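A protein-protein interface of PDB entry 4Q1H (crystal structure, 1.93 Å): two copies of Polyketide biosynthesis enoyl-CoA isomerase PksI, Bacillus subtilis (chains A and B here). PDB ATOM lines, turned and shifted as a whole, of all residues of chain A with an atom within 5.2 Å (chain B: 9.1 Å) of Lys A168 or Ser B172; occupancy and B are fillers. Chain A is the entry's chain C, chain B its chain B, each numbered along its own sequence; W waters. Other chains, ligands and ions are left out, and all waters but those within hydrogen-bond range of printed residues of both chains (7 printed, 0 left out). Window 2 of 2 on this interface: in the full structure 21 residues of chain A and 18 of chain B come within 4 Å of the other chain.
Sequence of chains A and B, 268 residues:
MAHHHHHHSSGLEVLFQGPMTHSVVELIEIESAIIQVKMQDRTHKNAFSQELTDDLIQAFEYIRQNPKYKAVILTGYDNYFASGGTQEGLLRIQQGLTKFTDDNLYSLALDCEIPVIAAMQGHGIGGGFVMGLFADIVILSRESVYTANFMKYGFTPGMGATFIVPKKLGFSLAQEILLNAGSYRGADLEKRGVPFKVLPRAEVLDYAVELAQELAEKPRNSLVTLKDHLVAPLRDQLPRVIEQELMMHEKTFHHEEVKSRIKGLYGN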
ATOM      1  N   LEU A 133      14.964  35.782  11.652  1.00  0.00           N
ATOM      2  CA  LEU A 133      14.650  35.129  12.922  1.00  0.00           C
ATOM      3  C   LEU A 133      13.922  33.796  12.772  1.00  0.00           C
ATOM      4  O   LEU A 133      13.980  32.946  13.677  1.00  0.00           O
ATOM      5  CB  LEU A 133      13.834  36.054  13.801  1.00  0.00           C
ATOM      6  CG  LEU A 133      14.643  37.240  14.385  1.00  0.00           C
ATOM      7  CD1 LEU A 133      13.651  38.108  15.243  1.00  0.00           C
ATOM      8  CD2 LEU A 133      15.835  36.771  15.201  1.00  0.00           C
ATOM      9  N   PHE A 134      13.231  33.602  11.635  1.00  0.00           N
ATOM     10  CA  PHE A 134      12.548  32.304  11.383  1.00  0.00           C
ATOM     11  C   PHE A 134      13.515  31.261  10.883  1.00  0.00           C
ATOM     12  O   PHE A 134      13.142  30.074  10.696  1.00  0.00           O
ATOM     13  CB  PHE A 134      11.408  32.453  10.343  1.00  0.00           C
ATOM     14  CG  PHE A 134      10.115  32.972  10.940  1.00  0.00           C
ATOM     15  CD1 PHE A 134       9.283  32.108  11.691  1.00  0.00           C
ATOM     16  CD2 PHE A 134       9.707  34.281  10.752  1.00  0.00           C
ATOM     17  CE1 PHE A 134       8.041  32.538  12.222  1.00  0.00           C
ATOM     18  CE2 PHE A 134       8.481  34.731  11.331  1.00  0.00           C
ATOM     19  CZ  PHE A 134       7.668  33.874  12.041  1.00  0.00           C
ATOM     20  N   ALA A 135      14.778  31.649  10.644  1.00  0.00           N
ATOM     21  CA  ALA A 135      15.758  30.612  10.330  1.00  0.00           C
ATOM     22  C   ALA A 135      16.085  29.718  11.550  1.00  0.00           C
ATOM     23  O   ALA A 135      15.913  30.106  12.679  1.00  0.00           O
ATOM     24  CB  ALA A 135      17.050  31.261   9.721  1.00  0.00           C
ATOM     25  N   ASP A 136      16.653  28.536  11.328  1.00  0.00           N
ATOM     26  CA  ASP A 136      16.929  27.627  12.432  1.00  0.00           C
ATOM     27  C   ASP A 136      18.135  28.122  13.232  1.00  0.00           C
ATOM     28  O   ASP A 136      18.213  27.804  14.421  1.00  0.00           O
ATOM     29  CB  ASP A 136      17.222  26.227  11.868  1.00  0.00           C
ATOM     30  CG  ASP A 136      16.011  25.784  10.988  1.00  0.00           C
ATOM     31  OD1 ASP A 136      14.962  25.467  11.627  1.00  0.00           O
ATOM     32  OD2 ASP A 136      16.062  25.935   9.742  1.00  0.00           O
ATOM     33  N   VAL A 138      20.696  31.591  13.749  1.00  0.00           N
ATOM     34  CA  VAL A 138      20.771  33.005  13.337  1.00  0.00           C
ATOM     35  C   VAL A 138      22.176  33.497  13.864  1.00  0.00           C
ATOM     36  O   VAL A 138      22.494  33.263  15.038  1.00  0.00           O
ATOM     37  CB  VAL A 138      19.686  33.784  14.057  1.00  0.00           C
ATOM     38  CG1 VAL A 138      19.819  35.258  13.695  1.00  0.00           C
ATOM     39  CG2 VAL A 138      18.256  33.306  13.686  1.00  0.00           C
ATOM     40  N   PHE A 163       5.260  36.694  17.448  1.00  0.00           N
ATOM     41  CA  PHE A 163       5.485  35.295  17.847  1.00  0.00           C
ATOM     42  C   PHE A 163       6.997  34.927  17.824  1.00  0.00           C
ATOM     43  O   PHE A 163       7.541  34.325  18.734  1.00  0.00           O
ATOM     44  CB  PHE A 163       4.771  34.374  16.834  1.00  0.00           C
ATOM     45  CG  PHE A 163       4.963  32.929  17.122  1.00  0.00           C
ATOM     46  CD1 PHE A 163       4.381  32.348  18.240  1.00  0.00           C
ATOM     47  CD2 PHE A 163       5.703  32.134  16.238  1.00  0.00           C
ATOM     48  CE1 PHE A 163       4.576  30.998  18.531  1.00  0.00           C
ATOM     49  CE2 PHE A 163       5.907  30.801  16.528  1.00  0.00           C
ATOM     50  CZ  PHE A 163       5.326  30.230  17.680  1.00  0.00           C
ATOM     51  N   ILE A 164       7.656  35.261  16.731  1.00  0.00           N
ATOM     52  CA  ILE A 164       9.052  34.717  16.565  1.00  0.00           C
ATOM     53  C   ILE A 164      10.031  35.495  17.441  1.00  0.00           C
ATOM     54  O   ILE A 164      11.039  34.969  17.869  1.00  0.00           O
ATOM     55  CB  ILE A 164       9.425  34.714  15.034  1.00  0.00           C
ATOM     56  CG1 ILE A 164      10.613  33.783  14.738  1.00  0.00           C
ATOM     57  CG2 ILE A 164       9.707  36.177  14.524  1.00  0.00           C
ATOM     58  CD1 ILE A 164      10.397  32.281  15.165  1.00  0.00           C
ATOM     59  N   VAL A 165       9.786  36.795  17.692  1.00  0.00           N
ATOM     60  CA  VAL A 165      10.714  37.499  18.545  1.00  0.00           C
ATOM     61  C   VAL A 165      10.749  36.941  19.970  1.00  0.00           C
ATOM     62  O   VAL A 165      11.824  36.634  20.487  1.00  0.00           O
ATOM     63  CB  VAL A 165      10.491  39.063  18.474  1.00  0.00           C
ATOM     64  CG1 VAL A 165      11.448  39.821  19.414  1.00  0.00           C
ATOM     65  CG2 VAL A 165      10.650  39.507  16.986  1.00  0.00           C
ATOM     66  N   PRO A 166       9.567  36.783  20.640  1.00  0.00           N
ATOM     67  CA  PRO A 166       9.696  36.152  21.949  1.00  0.00           C
ATOM     68  C   PRO A 166      10.218  34.680  21.830  1.00  0.00           C
ATOM     69  O   PRO A 166      10.897  34.179  22.750  1.00  0.00           O
ATOM     70  CB  PRO A 166       8.244  36.079  22.465  1.00  0.00           C
ATOM     71  CG  PRO A 166       7.373  36.879  21.493  1.00  0.00           C
ATOM     72  CD  PRO A 166       8.223  37.306  20.332  1.00  0.00           C
ATOM     73  N   LYS A 167       9.861  33.968  20.740  1.00  0.00           N
ATOM     74  CA  LYS A 167      10.261  32.524  20.670  1.00  0.00           C
ATOM     75  C   LYS A 167      11.792  32.432  20.642  1.00  0.00           C
ATOM     76  O   LYS A 167      12.425  31.586  21.301  1.00  0.00           O
ATOM     77  CB  LYS A 167       9.711  31.881  19.381  1.00  0.00           C
ATOM     78  CG  LYS A 167      10.078  30.395  19.294  1.00  0.00           C
ATOM     79  CD  LYS A 167       9.256  29.621  20.344  1.00  0.00           C
ATOM     80  CE  LYS A 167       9.318  28.116  20.156  1.00  0.00           C
ATOM     81  NZ  LYS A 167       8.474  27.230  21.089  1.00  0.00           N
ATOM     82  N   LYS A 168      12.419  33.320  19.872  1.00  0.00           N
ATOM     83  CA  LYS A 168      13.889  33.220  19.666  1.00  0.00           C
ATOM     84  C   LYS A 168      14.709  34.037  20.639  1.00  0.00           C
ATOM     85  O   LYS A 168      15.865  33.629  21.058  1.00  0.00           O
ATOM     86  CB  LYS A 168      14.260  33.707  18.234  1.00  0.00           C
ATOM     87  CG  LYS A 168      13.675  32.818  17.101  1.00  0.00           C
ATOM     88  CD  LYS A 168      14.328  31.381  17.177  1.00  0.00           C
ATOM     89  CE  LYS A 168      13.803  30.501  16.033  1.00  0.00           C
ATOM     90  NZ  LYS A 168      14.796  30.710  14.943  1.00  0.00           N
ATOM     91  N   LEU A 169      14.204  35.218  21.021  1.00  0.00           N
ATOM     92  CA  LEU A 169      14.962  36.074  21.996  1.00  0.00           C
ATOM     93  C   LEU A 169      14.467  36.078  23.433  1.00  0.00           C
ATOM     94  O   LEU A 169      15.063  36.779  24.264  1.00  0.00           O
ATOM     95  CB  LEU A 169      15.050  37.534  21.481  1.00  0.00           C
ATOM     96  CG  LEU A 169      15.797  37.628  20.139  1.00  0.00           C
ATOM     97  CD1 LEU A 169      15.898  39.003  19.680  1.00  0.00           C
ATOM     98  CD2 LEU A 169      17.204  37.036  20.291  1.00  0.00           C
ATOM     99  N   GLY A 170      13.347  35.383  23.727  1.00  0.00           N
ATOM    100  CA  GLY A 170      12.791  35.259  25.072  1.00  0.00           C
ATOM    101  C   GLY A 170      11.748  36.324  25.303  1.00  0.00           C
ATOM    102  O   GLY A 170      11.764  37.393  24.700  1.00  0.00           O
ATOM    103  N   PRO A 195      21.061  34.370  22.565  1.00  0.00           N
ATOM    104  CA  PRO A 195      21.676  33.039  22.333  1.00  0.00           C
ATOM    105  C   PRO A 195      22.340  32.920  20.955  1.00  0.00           C
ATOM    106  O   PRO A 195      22.986  31.904  20.647  1.00  0.00           O
ATOM    107  CB  PRO A 195      20.461  32.099  22.381  1.00  0.00           C
ATOM    108  CG  PRO A 195      19.234  32.968  21.977  1.00  0.00           C
ATOM    109  CD  PRO A 195      19.559  34.307  22.632  1.00  0.00           C
ATOM    110  N   PHE A 196      22.156  33.907  20.094  1.00  0.00           N
ATOM    111  CA  PHE A 196      22.766  33.936  18.743  1.00  0.00           C
ATOM    112  C   PHE A 196      24.247  34.196  18.847  1.00  0.00           C
ATOM    113  O   PHE A 196      24.696  35.015  19.664  1.00  0.00           O
ATOM    114  CB  PHE A 196      22.199  35.142  17.919  1.00  0.00           C
ATOM    115  CG  PHE A 196      20.685  35.113  17.769  1.00  0.00           C
ATOM    116  CD1 PHE A 196      19.962  33.928  17.925  1.00  0.00           C
ATOM    117  CD2 PHE A 196      19.992  36.313  17.535  1.00  0.00           C
ATOM    118  CE1 PHE A 196      18.572  33.918  17.767  1.00  0.00           C
ATOM    119  CE2 PHE A 196      18.601  36.303  17.389  1.00  0.00           C
ATOM    120  CZ  PHE A 196      17.895  35.124  17.471  1.00  0.00           C
ATOM    121  N   LEU A 234       5.925  25.911  15.919  1.00  0.00           N
ATOM    122  CA  LEU A 234       5.965  27.187  15.167  1.00  0.00           C
ATOM    123  C   LEU A 234       5.102  27.156  13.899  1.00  0.00           C
ATOM    124  O   LEU A 234       4.302  28.018  13.678  1.00  0.00           O
ATOM    125  CB  LEU A 234       7.431  27.535  14.749  1.00  0.00           C
ATOM    126  CG  LEU A 234       8.384  27.988  15.900  1.00  0.00           C
ATOM    127  CD1 LEU A 234       8.679  26.856  16.868  1.00  0.00           C
ATOM    128  CD2 LEU A 234       9.659  28.523  15.253  1.00  0.00           C
ATOM    129  N   VAL B 165      16.597  20.127  26.469  1.00  0.00           N
ATOM    130  CA  VAL B 165      17.605  21.133  25.994  1.00  0.00           C
ATOM    131  C   VAL B 165      16.944  22.528  25.749  1.00  0.00           C
ATOM    132  O   VAL B 165      17.443  23.530  26.276  1.00  0.00           O
ATOM    133  CB  VAL B 165      18.422  20.621  24.750  1.00  0.00           C
ATOM    134  CG1 VAL B 165      19.479  21.694  24.282  1.00  0.00           C
ATOM    135  CG2 VAL B 165      19.188  19.349  25.213  1.00  0.00           C
ATOM    136  N   PRO B 166      15.812  22.580  25.040  1.00  0.00           N
ATOM    137  CA  PRO B 166      15.220  23.893  24.894  1.00  0.00           C
ATOM    138  C   PRO B 166      14.642  24.403  26.215  1.00  0.00           C
ATOM    139  O   PRO B 166      14.630  25.617  26.439  1.00  0.00           O
ATOM    140  CB  PRO B 166      14.108  23.704  23.823  1.00  0.00           C
ATOM    141  CG  PRO B 166      14.108  22.226  23.419  1.00  0.00           C
ATOM    142  CD  PRO B 166      15.217  21.527  24.153  1.00  0.00           C
ATOM    143  N   LYS B 167      14.125  23.516  27.067  1.00  0.00           N
ATOM    144  CA  LYS B 167      13.499  24.016  28.309  1.00  0.00           C
ATOM    145  C   LYS B 167      14.638  24.682  29.134  1.00  0.00           C
ATOM    146  O   LYS B 167      14.400  25.684  29.766  1.00  0.00           O
ATOM    147  CB  LYS B 167      12.940  22.837  29.175  1.00  0.00           C
ATOM    148  CG  LYS B 167      12.185  23.374  30.454  1.00  0.00           C
ATOM    149  CD  LYS B 167      11.014  24.140  29.851  1.00  0.00           C
ATOM    150  CE  LYS B 167       9.743  24.040  30.658  1.00  0.00           C
ATOM    151  NZ  LYS B 167       8.711  24.571  29.751  1.00  0.00           N
ATOM    152  N   LEU B 169      18.059  25.494  28.068  1.00  0.00           N
ATOM    153  CA  LEU B 169      18.939  26.462  27.372  1.00  0.00           C
ATOM    154  C   LEU B 169      18.248  27.385  26.358  1.00  0.00           C
ATOM    155  O   LEU B 169      18.943  28.234  25.754  1.00  0.00           O
ATOM    156  CB  LEU B 169      20.080  25.680  26.661  1.00  0.00           C
ATOM    157  CG  LEU B 169      20.920  24.854  27.617  1.00  0.00           C
ATOM    158  CD1 LEU B 169      22.027  24.178  26.872  1.00  0.00           C
ATOM    159  CD2 LEU B 169      21.494  25.764  28.707  1.00  0.00           C
ATOM    160  N   GLY B 170      16.923  27.238  26.158  1.00  0.00           N
ATOM    161  CA  GLY B 170      16.132  28.171  25.323  1.00  0.00           C
ATOM    162  C   GLY B 170      16.006  27.495  23.924  1.00  0.00           C
ATOM    163  O   GLY B 170      16.911  26.776  23.465  1.00  0.00           O
ATOM    164  N   PHE B 171      14.960  27.874  23.223  1.00  0.00           N
ATOM    165  CA  PHE B 171      14.673  27.268  21.915  1.00  0.00           C
ATOM    166  C   PHE B 171      15.844  27.533  20.947  1.00  0.00           C
ATOM    167  O   PHE B 171      16.278  26.617  20.205  1.00  0.00           O
ATOM    168  CB  PHE B 171      13.424  27.945  21.367  1.00  0.00           C
ATOM    169  CG  PHE B 171      13.009  27.399  20.016  1.00  0.00           C
ATOM    170  CD1 PHE B 171      12.326  26.198  19.944  1.00  0.00           C
ATOM    171  CD2 PHE B 171      13.375  28.047  18.852  1.00  0.00           C
ATOM    172  CE1 PHE B 171      11.962  25.647  18.692  1.00  0.00           C
ATOM    173  CE2 PHE B 171      13.039  27.517  17.644  1.00  0.00           C
ATOM    174  CZ  PHE B 171      12.302  26.318  17.562  1.00  0.00           C
ATOM    175  N   SER B 172      16.372  28.765  20.857  1.00  0.00           N
ATOM    176  CA  SER B 172      17.373  29.054  19.796  1.00  0.00           C
ATOM    177  C   SER B 172      18.675  28.237  19.923  1.00  0.00           C
ATOM    178  O   SER B 172      19.134  27.588  18.948  1.00  0.00           O
ATOM    179  CB  SER B 172      17.721  30.579  19.679  1.00  0.00           C
ATOM    180  OG  SER B 172      18.787  30.835  18.745  1.00  0.00           O
ATOM    181  N   LEU B 173      19.281  28.306  21.083  1.00  0.00           N
ATOM    182  CA  LEU B 173      20.518  27.567  21.301  1.00  0.00           C
ATOM    183  C   LEU B 173      20.251  26.061  21.149  1.00  0.00           C
ATOM    184  O   LEU B 173      21.144  25.330  20.594  1.00  0.00           O
ATOM    185  CB  LEU B 173      21.099  27.902  22.664  1.00  0.00           C
ATOM    186  CG  LEU B 173      22.511  27.357  22.898  1.00  0.00           C
ATOM    187  CD1 LEU B 173      23.493  27.885  21.831  1.00  0.00           C
ATOM    188  CD2 LEU B 173      22.990  27.857  24.304  1.00  0.00           C
ATOM    189  N   ALA B 174      19.086  25.573  21.613  1.00  0.00           N
ATOM    190  CA  ALA B 174      18.771  24.122  21.468  1.00  0.00           C
ATOM    191  C   ALA B 174      18.777  23.701  19.971  1.00  0.00           C
ATOM    192  O   ALA B 174      19.199  22.592  19.677  1.00  0.00           O
ATOM    193  CB  ALA B 174      17.378  23.798  22.069  1.00  0.00           C
ATOM    194  N   GLN B 175      18.278  24.543  19.026  1.00  0.00           N
ATOM    195  CA  GLN B 175      18.229  24.124  17.619  1.00  0.00           C
ATOM    196  C   GLN B 175      19.646  23.789  17.178  1.00  0.00           C
ATOM    197  O   GLN B 175      19.831  22.775  16.516  1.00  0.00           O
ATOM    198  CB  GLN B 175      17.693  25.224  16.652  1.00  0.00           C
ATOM    199  CG  GLN B 175      16.400  25.860  17.137  1.00  0.00           C
ATOM    200  CD  GLN B 175      15.346  24.834  17.350  1.00  0.00           C
ATOM    201  OE1 GLN B 175      14.986  24.457  18.511  1.00  0.00           O
ATOM    202  NE2 GLN B 175      14.872  24.301  16.260  1.00  0.00           N
ATOM    203  N   GLU B 176      20.620  24.668  17.508  1.00  0.00           N
ATOM    204  CA  GLU B 176      21.960  24.475  17.013  1.00  0.00           C
ATOM    205  C   GLU B 176      22.585  23.257  17.743  1.00  0.00           C
ATOM    206  O   GLU B 176      23.173  22.375  17.143  1.00  0.00           O
ATOM    207  CB  GLU B 176      22.758  25.728  17.482  1.00  0.00           C
ATOM    208  CG  GLU B 176      24.187  25.648  17.153  1.00  0.00           C
ATOM    209  CD  GLU B 176      24.901  26.928  17.700  1.00  0.00           C
ATOM    210  OE1 GLU B 176      24.285  28.023  17.504  1.00  0.00           O
ATOM    211  OE2 GLU B 176      26.030  26.764  18.272  1.00  0.00           O
ATOM    212  N   ILE B 177      22.357  23.189  19.068  1.00  0.00           N
ATOM    213  CA  ILE B 177      22.902  22.013  19.770  1.00  0.00           C
ATOM    214  C   ILE B 177      22.397  20.655  19.233  1.00  0.00           C
ATOM    215  O   ILE B 177      23.192  19.719  19.069  1.00  0.00           O
ATOM    216  CB  ILE B 177      22.583  22.155  21.296  1.00  0.00           C
ATOM    217  CG1 ILE B 177      23.542  23.212  21.834  1.00  0.00           C
ATOM    218  CG2 ILE B 177      22.736  20.807  22.039  1.00  0.00           C
ATOM    219  CD1 ILE B 177      23.009  23.664  23.229  1.00  0.00           C
ATOM    220  N   LEU B 178      21.087  20.576  18.981  1.00  0.00           N
ATOM    221  CA  LEU B 178      20.459  19.274  18.662  1.00  0.00           C
ATOM    222  C   LEU B 178      20.677  18.932  17.173  1.00  0.00           C
ATOM    223  O   LEU B 178      21.007  17.796  16.882  1.00  0.00           O
ATOM    224  CB  LEU B 178      18.924  19.380  18.890  1.00  0.00           C
ATOM    225  CG  LEU B 178      18.675  19.489  20.407  1.00  0.00           C
ATOM    226  CD1 LEU B 178      17.167  19.881  20.576  1.00  0.00           C
ATOM    227  CD2 LEU B 178      18.925  18.170  21.118  1.00  0.00           C
ATOM    228  N   LEU B 179      20.515  19.926  16.276  1.00  0.00           N
ATOM    229  CA  LEU B 179      20.662  19.652  14.831  1.00  0.00           C
ATOM    230  C   LEU B 179      22.128  19.320  14.480  1.00  0.00           C
ATOM    231  O   LEU B 179      22.413  18.417  13.666  1.00  0.00           O
ATOM    232  CB  LEU B 179      20.240  20.925  14.008  1.00  0.00           C
ATOM    233  CG  LEU B 179      18.720  21.130  13.853  1.00  0.00           C
ATOM    234  CD1 LEU B 179      18.616  22.544  13.232  1.00  0.00           C
ATOM    235  CD2 LEU B 179      18.191  20.077  12.860  1.00  0.00           C
ATOM    236  N   TYR B 184      30.920  21.629  22.755  1.00  0.00           N
ATOM    237  CA  TYR B 184      31.175  22.991  23.300  1.00  0.00           C
ATOM    238  C   TYR B 184      31.948  22.835  24.619  1.00  0.00           C
ATOM    239  O   TYR B 184      31.562  22.036  25.471  1.00  0.00           O
ATOM    240  CB  TYR B 184      29.844  23.691  23.678  1.00  0.00           C
ATOM    241  CG  TYR B 184      28.899  23.851  22.516  1.00  0.00           C
ATOM    242  CD1 TYR B 184      28.730  25.112  21.910  1.00  0.00           C
ATOM    243  CD2 TYR B 184      28.166  22.727  21.981  1.00  0.00           C
ATOM    244  CE1 TYR B 184      27.874  25.258  20.857  1.00  0.00           C
ATOM    245  CE2 TYR B 184      27.316  22.879  20.894  1.00  0.00           C
ATOM    246  CZ  TYR B 184      27.165  24.120  20.323  1.00  0.00           C
ATOM    247  OH  TYR B 184      26.275  24.295  19.223  1.00  0.00           O
ATOM    248  N   ARG B 192      28.107  32.008  25.265  1.00  0.00           N
ATOM    249  CA  ARG B 192      26.831  32.111  24.535  1.00  0.00           C
ATOM    250  C   ARG B 192      25.664  32.543  25.420  1.00  0.00           C
ATOM    251  O   ARG B 192      24.552  32.709  24.950  1.00  0.00           O
ATOM    252  CB  ARG B 192      26.506  30.779  23.832  1.00  0.00           C
ATOM    253  CG  ARG B 192      27.552  30.312  22.810  1.00  0.00           C
ATOM    254  CD  ARG B 192      27.691  31.263  21.607  1.00  0.00           C
ATOM    255  NE  ARG B 192      26.465  31.178  20.834  1.00  0.00           N
ATOM    256  CZ  ARG B 192      26.098  30.212  20.004  1.00  0.00           C
ATOM    257  NH1 ARG B 192      26.953  29.200  19.661  1.00  0.00           N
ATOM    258  NH2 ARG B 192      24.854  30.247  19.468  1.00  0.00           N
HETATM  259  O   HOH W   1      23.899  31.386  16.377  1.00  0.00           O
HETATM  260  O   HOH W   2      15.165  23.524  13.770  1.00  0.00           O
HETATM  261  O   HOH W   3      21.111  30.241  19.267  1.00  0.00           O
HETATM  262  O   HOH W   4      15.740  31.102  22.448  1.00  0.00           O
HETATM  263  O   HOH W   5      19.960  28.109  16.635  1.00  0.00           O
HETATM  264  O   HOH W   6      14.670  26.148  14.586  1.00  0.00           O
HETATM  265  O   HOH W   7      25.325  33.540  22.006  1.00  0.00           O
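Of the 16 printed residues of chain B, 4 touch a printed residue of chain A.
Hydrophobic or aromatic side chains of chain B within 4 Å of the printed part of chain A: Phe B171.
Of the 16 printed residues of chain A, 6 touch a printed residue of chain B.
Among the printed residues, 8 pairs touch across the chains.
Among the printed residues, no Asp or Glu carboxylate lies within 4 Å of a Lys or Arg side-chain nitrogen of the other chain.
Water W3 lies within hydrogen-bond range of the side-chain hydroxyl of Ser B172, the backbone carbonyl oxygen of Pro A195 and the backbone NH of Leu B173.
Water W6 lies within hydrogen-bond range of the side-chain amide nitrogen of Gln B175 (2.5 Å) and the side-chain carboxylate of Asp A136 (3.1 Å).
Water W5 bridges O of Ser B172 (2.5 Å) and O of Asp A136 (2.8 Å).
Water W2 bridges NE2 of Gln B175 (2.6 Å) and OD1 of Asp A136 (2.9 Å).
Water W7 lies within hydrogen-bond range of O of Phe A196, NE of Arg B192 and O of Pro A195.
Water W4 lies within hydrogen-bond range of the backbone carbonyl oxygen (O) of Lys A168, the backbone NH (N) of Ser B172 and the backbone NH (N) of Phe B171.
Gln B175 touches Asp A136 (CB to O, 3.5 Å).
Phe B171 touches Lys A167 (CD1 to CE, 3.6 Å).
CE of Lys A168 touches CE2 of Phe B171, at 3.5 Å.
Ser B172 touches Lys A168 (CB to O, 3.8 Å).
Ser B172 touches Pro A195 (CB to CG, 3.6 Å).
Ser B172 touches Phe A196 (OG to CE1, 3.2 Å).
Leu A234 touches Phe B171 (CD1 to CZ, 3.7 Å).
The guanidinium group (NH2) of Arg B192 is in hydrogen-bond range of the backbone carbonyl oxygen (O) of Pro A195 (2.8 Å).
Of the printed residues of chain B, Lys A168 touches Phe B171 and Ser B172.
Of the printed residues of chain A, Ser B172 touches Lys A168, Pro A195 and Phe A196.
Of the printed residues of chain B, Asp A136 touches Gln B175 (3.5 Å).
Of the printed residues of chain B, Lys A167 touches Phe B171.
Printed residues of chain B within 4 Å of Leu A234: Phe B171.
Printed residues of chain B within 4 Å of Pro A195: Ser B172 (3.6 Å) and Arg B192 (2.8 Å).
Of the printed residues of chain A, Arg B192 touches Pro A195.
Gly B170 touches none of the printed residues of chain A.
NZ of Lys A168 lies within hydrogen-bond range of O of Ala A135 (2.6 Å).
OE1 of Gln B175 sits close to O of Phe B171, 3.0 Å away.
OE2 of Glu B176 is in salt-bridge range of NH1 of Arg B192.
O of Leu A133 is in hydrogen-bond range of NZ of Lys A168 (2.7 Å).
Positions printed for both chains: 165, 166, 167, 169 and 170.
Of the 8 pairs that touch across the chains among the printed residues, none has its exchanged pair printed and touching as well.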
